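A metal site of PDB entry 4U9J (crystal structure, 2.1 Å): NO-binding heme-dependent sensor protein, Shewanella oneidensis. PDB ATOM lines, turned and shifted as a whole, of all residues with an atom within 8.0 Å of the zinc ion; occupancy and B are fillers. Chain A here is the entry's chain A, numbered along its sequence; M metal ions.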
ATOM      1  N   TYR A 132      12.041 -28.719  -6.467  1.00  0.00           N
ATOM      2  CA  TYR A 132      12.320 -30.157  -6.529  1.00  0.00           C
ATOM      3  C   TYR A 132      12.731 -30.620  -5.134  1.00  0.00           C
ATOM      4  O   TYR A 132      13.516 -29.964  -4.461  1.00  0.00           O
ATOM      5  CB  TYR A 132      13.457 -30.423  -7.505  1.00  0.00           C
ATOM      6  CG  TYR A 132      14.046 -31.797  -7.450  1.00  0.00           C
ATOM      7  CD1 TYR A 132      15.077 -32.108  -6.565  1.00  0.00           C
ATOM      8  CD2 TYR A 132      13.610 -32.807  -8.279  1.00  0.00           C
ATOM      9  CE1 TYR A 132      15.609 -33.399  -6.523  1.00  0.00           C
ATOM     10  CE2 TYR A 132      14.171 -34.073  -8.257  1.00  0.00           C
ATOM     11  CZ  TYR A 132      15.146 -34.378  -7.365  1.00  0.00           C
ATOM     12  OH  TYR A 132      15.724 -35.646  -7.321  1.00  0.00           O
ATOM     13  N   ARG A 137      18.088 -36.969  -4.235  1.00  0.00           N
ATOM     14  CA  ARG A 137      18.918 -35.782  -4.586  1.00  0.00           C
ATOM     15  C   ARG A 137      19.419 -35.812  -6.040  1.00  0.00           C
ATOM     16  O   ARG A 137      20.590 -35.535  -6.327  1.00  0.00           O
ATOM     17  CB  ARG A 137      20.071 -35.658  -3.583  1.00  0.00           C
ATOM     18  CG  ARG A 137      19.518 -35.529  -2.179  1.00  0.00           C
ATOM     19  CD  ARG A 137      20.470 -34.814  -1.202  1.00  0.00           C
ATOM     20  NE  ARG A 137      21.725 -35.536  -1.121  1.00  0.00           N
ATOM     21  CZ  ARG A 137      22.707 -35.185  -0.318  1.00  0.00           C
ATOM     22  NH1 ARG A 137      22.561 -34.144   0.475  1.00  0.00           N
ATOM     23  NH2 ARG A 137      23.835 -35.888  -0.291  1.00  0.00           N
ATOM     24  N   LEU A 138      18.508 -36.108  -6.955  1.00  0.00           N
ATOM     25  CA  LEU A 138      18.832 -36.211  -8.379  1.00  0.00           C
ATOM     26  C   LEU A 138      18.452 -34.915  -9.148  1.00  0.00           C
ATOM     27  O   LEU A 138      17.950 -34.980 -10.274  1.00  0.00           O
ATOM     28  CB  LEU A 138      18.129 -37.439  -8.970  1.00  0.00           C
ATOM     29  CG  LEU A 138      18.830 -38.764  -8.641  1.00  0.00           C
ATOM     30  CD1 LEU A 138      17.952 -40.011  -9.004  1.00  0.00           C
ATOM     31  CD2 LEU A 138      20.172 -38.819  -9.428  1.00  0.00           C
ATOM     32  N   CYS A 139      18.645 -33.751  -8.505  1.00  0.00           N
ATOM     33  CA  CYS A 139      18.279 -32.460  -9.108  1.00  0.00           C
ATOM     34  C   CYS A 139      19.045 -32.217 -10.405  1.00  0.00           C
ATOM     35  O   CYS A 139      18.568 -31.504 -11.251  1.00  0.00           O
ATOM     36  CB  CYS A 139      18.548 -31.290  -8.157  1.00  0.00           C
ATOM     37  SG  CYS A 139      20.264 -31.349  -7.469  1.00  0.00           S
ATOM     38  N   PHE A 140      20.232 -32.789 -10.546  1.00  0.00           N
ATOM     39  CA  PHE A 140      20.967 -32.605 -11.761  1.00  0.00           C
ATOM     40  C   PHE A 140      20.424 -33.490 -12.865  1.00  0.00           C
ATOM     41  O   PHE A 140      20.523 -33.130 -14.049  1.00  0.00           O
ATOM     42  CB  PHE A 140      22.460 -32.830 -11.548  1.00  0.00           C
ATOM     43  CG  PHE A 140      23.112 -31.693 -10.774  1.00  0.00           C
ATOM     44  CD1 PHE A 140      23.532 -30.550 -11.431  1.00  0.00           C
ATOM     45  CD2 PHE A 140      23.247 -31.735  -9.388  1.00  0.00           C
ATOM     46  CE1 PHE A 140      24.118 -29.459 -10.735  1.00  0.00           C
ATOM     47  CE2 PHE A 140      23.825 -30.643  -8.703  1.00  0.00           C
ATOM     48  CZ  PHE A 140      24.262 -29.514  -9.383  1.00  0.00           C
ATOM     49  N   ALA A 142      17.279 -33.891 -12.979  1.00  0.00           N
ATOM     50  CA  ALA A 142      16.145 -33.046 -13.346  1.00  0.00           C
ATOM     51  C   ALA A 142      16.529 -31.919 -14.271  1.00  0.00           C
ATOM     52  O   ALA A 142      15.747 -31.648 -15.195  1.00  0.00           O
ATOM     53  CB  ALA A 142      15.485 -32.465 -12.120  1.00  0.00           C
ATOM     54  N   GLU A 143      17.706 -31.254 -14.026  1.00  0.00           N
ATOM     55  CA  GLU A 143      18.187 -30.249 -14.979  1.00  0.00           C
ATOM     56  C   GLU A 143      18.317 -30.824 -16.373  1.00  0.00           C
ATOM     57  O   GLU A 143      17.845 -30.251 -17.331  1.00  0.00           O
ATOM     58  CB  GLU A 143      19.567 -29.640 -14.600  1.00  0.00           C
ATOM     59  CG  GLU A 143      19.453 -28.525 -13.684  1.00  0.00           C
ATOM     60  CD  GLU A 143      20.719 -27.651 -13.651  1.00  0.00           C
ATOM     61  OE1 GLU A 143      20.957 -27.179 -12.543  1.00  0.00           O
ATOM     62  OE2 GLU A 143      21.389 -27.452 -14.657  1.00  0.00           O
ATOM     63  N   HIS A 161      20.189 -22.591 -10.402  1.00  0.00           N
ATOM     64  CA  HIS A 161      20.027 -23.649  -9.427  1.00  0.00           C
ATOM     65  C   HIS A 161      20.801 -23.253  -8.153  1.00  0.00           C
ATOM     66  O   HIS A 161      21.828 -23.848  -7.837  1.00  0.00           O
ATOM     67  CB  HIS A 161      20.577 -24.903 -10.070  1.00  0.00           C
ATOM     68  CG  HIS A 161      20.342 -26.170  -9.313  1.00  0.00           C
ATOM     69  ND1 HIS A 161      20.557 -27.392  -9.905  1.00  0.00           N
ATOM     70  CD2 HIS A 161      19.992 -26.438  -8.040  1.00  0.00           C
ATOM     71  CE1 HIS A 161      20.306 -28.354  -9.042  1.00  0.00           C
ATOM     72  NE2 HIS A 161      19.954 -27.803  -7.901  1.00  0.00           N
ATOM     73  N   ASP A 162      20.331 -22.206  -7.488  1.00  0.00           N
ATOM     74  CA  ASP A 162      21.085 -21.617  -6.371  1.00  0.00           C
ATOM     75  C   ASP A 162      20.620 -21.975  -4.972  1.00  0.00           C
ATOM     76  O   ASP A 162      21.262 -21.649  -4.048  1.00  0.00           O
ATOM     77  CB  ASP A 162      21.107 -20.087  -6.503  1.00  0.00           C
ATOM     78  CG  ASP A 162      21.739 -19.631  -7.816  1.00  0.00           C
ATOM     79  OD1 ASP A 162      22.779 -20.229  -8.177  1.00  0.00           O
ATOM     80  OD2 ASP A 162      21.163 -18.748  -8.513  1.00  0.00           O
ATOM     81  N   THR A 163      19.523 -22.686  -4.837  1.00  0.00           N
ATOM     82  CA  THR A 163      19.124 -23.384  -3.620  1.00  0.00           C
ATOM     83  C   THR A 163      19.197 -24.831  -3.998  1.00  0.00           C
ATOM     84  O   THR A 163      18.603 -25.216  -5.052  1.00  0.00           O
ATOM     85  CB  THR A 163      17.693 -23.044  -3.216  1.00  0.00           C
ATOM     86  OG1 THR A 163      17.639 -21.636  -3.050  1.00  0.00           O
ATOM     87  CG2 THR A 163      17.249 -23.696  -1.952  1.00  0.00           C
ATOM     88  N   CYS A 164      19.910 -25.636  -3.203  1.00  0.00           N
ATOM     89  CA  CYS A 164      20.166 -27.023  -3.607  1.00  0.00           C
ATOM     90  C   CYS A 164      20.325 -27.883  -2.372  1.00  0.00           C
ATOM     91  O   CYS A 164      20.887 -27.459  -1.326  1.00  0.00           O
ATOM     92  CB  CYS A 164      21.397 -27.096  -4.525  1.00  0.00           C
ATOM     93  SG  CYS A 164      21.818 -28.752  -5.030  1.00  0.00           S
ATOM     94  N   MET A 165      19.821 -29.094  -2.482  1.00  0.00           N
ATOM     95  CA  MET A 165      19.910 -30.028  -1.394  1.00  0.00           C
ATOM     96  C   MET A 165      21.388 -30.384  -1.126  1.00  0.00           C
ATOM     97  O   MET A 165      21.750 -30.757  -0.034  1.00  0.00           O
ATOM     98  CB  MET A 165      19.092 -31.299  -1.716  1.00  0.00           C
ATOM     99  CG  MET A 165      17.559 -31.052  -1.924  1.00  0.00           C
ATOM    100  SD  MET A 165      16.611 -32.597  -2.177  1.00  0.00           S
ATOM    101  CE  MET A 165      16.561 -33.208  -0.499  1.00  0.00           C
ATOM    102  N   HIS A 166      22.217 -30.332  -2.157  1.00  0.00           N
ATOM    103  CA  HIS A 166      23.618 -30.663  -2.015  1.00  0.00           C
ATOM    104  C   HIS A 166      24.385 -29.562  -1.259  1.00  0.00           C
ATOM    105  O   HIS A 166      25.480 -29.821  -0.819  1.00  0.00           O
ATOM    106  CB  HIS A 166      24.251 -30.951  -3.376  1.00  0.00           C
ATOM    107  CG  HIS A 166      23.759 -32.238  -4.006  1.00  0.00           C
ATOM    108  ND1 HIS A 166      24.196 -33.493  -3.614  1.00  0.00           N
ATOM    109  CD2 HIS A 166      22.816 -32.455  -4.962  1.00  0.00           C
ATOM    110  CE1 HIS A 166      23.565 -34.404  -4.316  1.00  0.00           C
ATOM    111  NE2 HIS A 166      22.740 -33.802  -5.139  1.00  0.00           N
ATOM    112  N   THR A 167      23.771 -28.376  -1.115  1.00  0.00           N
ATOM    113  CA  THR A 167      24.399 -27.219  -0.375  1.00  0.00           C
ATOM    114  C   THR A 167      23.587 -26.987   0.869  1.00  0.00           C
ATOM    115  O   THR A 167      23.643 -25.942   1.447  1.00  0.00           O
ATOM    116  CB  THR A 167      24.502 -25.926  -1.180  1.00  0.00           C
ATOM    117  OG1 THR A 167      23.216 -25.459  -1.612  1.00  0.00           O
ATOM    118  CG2 THR A 167      25.378 -26.124  -2.354  1.00  0.00           C
ATOM    119  N   ALA A 169      20.071 -27.348   1.695  1.00  0.00           N
ATOM    120  CA  ALA A 169      18.617 -27.079   1.757  1.00  0.00           C
ATOM    121  C   ALA A 169      17.848 -28.404   1.750  1.00  0.00           C
ATOM    122  O   ALA A 169      18.426 -29.454   1.483  1.00  0.00           O
ATOM    123  CB  ALA A 169      18.223 -26.163   0.597  1.00  0.00           C
ATOM    124  N   HIS A 171      15.337 -28.780  -0.288  1.00  0.00           N
ATOM    125  CA  HIS A 171      14.759 -28.821  -1.638  1.00  0.00           C
ATOM    126  C   HIS A 171      15.747 -28.070  -2.550  1.00  0.00           C
ATOM    127  O   HIS A 171      16.686 -27.375  -2.053  1.00  0.00           O
ATOM    128  CB  HIS A 171      13.413 -28.157  -1.646  1.00  0.00           C
ATOM    129  CG  HIS A 171      13.482 -26.686  -1.357  1.00  0.00           C
ATOM    130  ND1 HIS A 171      13.589 -26.169  -0.076  1.00  0.00           N
ATOM    131  CD2 HIS A 171      13.520 -25.613  -2.192  1.00  0.00           C
ATOM    132  CE1 HIS A 171      13.652 -24.852  -0.140  1.00  0.00           C
ATOM    133  NE2 HIS A 171      13.619 -24.483  -1.410  1.00  0.00           N
ATOM    134  N   CYS A 172      15.574 -28.197  -3.858  1.00  0.00           N
ATOM    135  CA  CYS A 172      16.254 -27.337  -4.813  1.00  0.00           C
ATOM    136  C   CYS A 172      15.269 -26.390  -5.507  1.00  0.00           C
ATOM    137  O   CYS A 172      14.102 -26.748  -5.682  1.00  0.00           O
ATOM    138  CB  CYS A 172      16.979 -28.184  -5.851  1.00  0.00           C
ATOM    139  SG  CYS A 172      18.062 -29.480  -5.249  1.00  0.00           S
ATOM    140  N   MET A 173      15.721 -25.183  -5.864  1.00  0.00           N
ATOM    141  CA  MET A 173      14.951 -24.285  -6.689  1.00  0.00           C
ATOM    142  C   MET A 173      15.633 -24.202  -8.058  1.00  0.00           C
ATOM    143  O   MET A 173      16.803 -23.841  -8.151  1.00  0.00           O
ATOM    144  CB  MET A 173      14.822 -22.899  -6.070  1.00  0.00           C
ATOM    145  CG  MET A 173      13.869 -22.820  -4.891  1.00  0.00           C
ATOM    146  SD  MET A 173      12.112 -23.316  -5.173  1.00  0.00           S
ATOM    147  CE  MET A 173      11.602 -22.278  -6.511  1.00  0.00           C
ATOM    148  N   LEU A 174      14.911 -24.584  -9.104  1.00  0.00           N
ATOM    149  CA  LEU A 174      15.405 -24.450 -10.479  1.00  0.00           C
ATOM    150  C   LEU A 174      14.627 -23.352 -11.150  1.00  0.00           C
ATOM    151  O   LEU A 174      13.444 -23.471 -11.375  1.00  0.00           O
ATOM    152  CB  LEU A 174      15.263 -25.744 -11.277  1.00  0.00           C
ATOM    153  CG  LEU A 174      16.331 -26.821 -11.047  1.00  0.00           C
ATOM    154  CD1 LEU A 174      16.508 -27.100  -9.684  1.00  0.00           C
ATOM    155  CD2 LEU A 174      15.866 -28.145 -11.594  1.00  0.00           C
HETATM  156 ZN    ZN M   1      19.975 -29.244  -6.444  1.00  0.00          ZN
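The backbone NH (N) of His 166 lies close to the side-chain sulfur (SG) of Cys 164 (3.3 Å). The backbone NH (N) of Met 165 sits close to the side-chain sulfur (SG) of Cys 172. N of Cys 172 lies within hydrogen-bond range of O of Tyr 132. The side-chain carboxylate of Glu 143 sits at hydrogen-bond distance from a ring nitrogen (ND1) of His 161 (2.7 Å). O of Cys 164 is in hydrogen-bond range of N of Ala 169 (3.1 Å). O of Cys 164 sits at hydrogen-bond distance from OG1 of Thr 167, 3.1 Å away.
Residues that only touch the zinc ion: Met 165. Five residues have an atom within 4 Å of the zinc ion: Cys 139, His 161, Cys 164, Met 165 and Cys 172. The nearest printed residue that does not touch the zinc ion is Thr 163 (4.5 Å).
The zinc ion is bound by a ring nitrogen (NE2) of His 161 (2.0 Å), the side-chain sulfur (SG) of Cys 172 (2.3 Å), the side-chain sulfur (SG) of Cys 139 (2.4 Å) and the side-chain sulfur (SG) of Cys 164 (2.4 Å).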
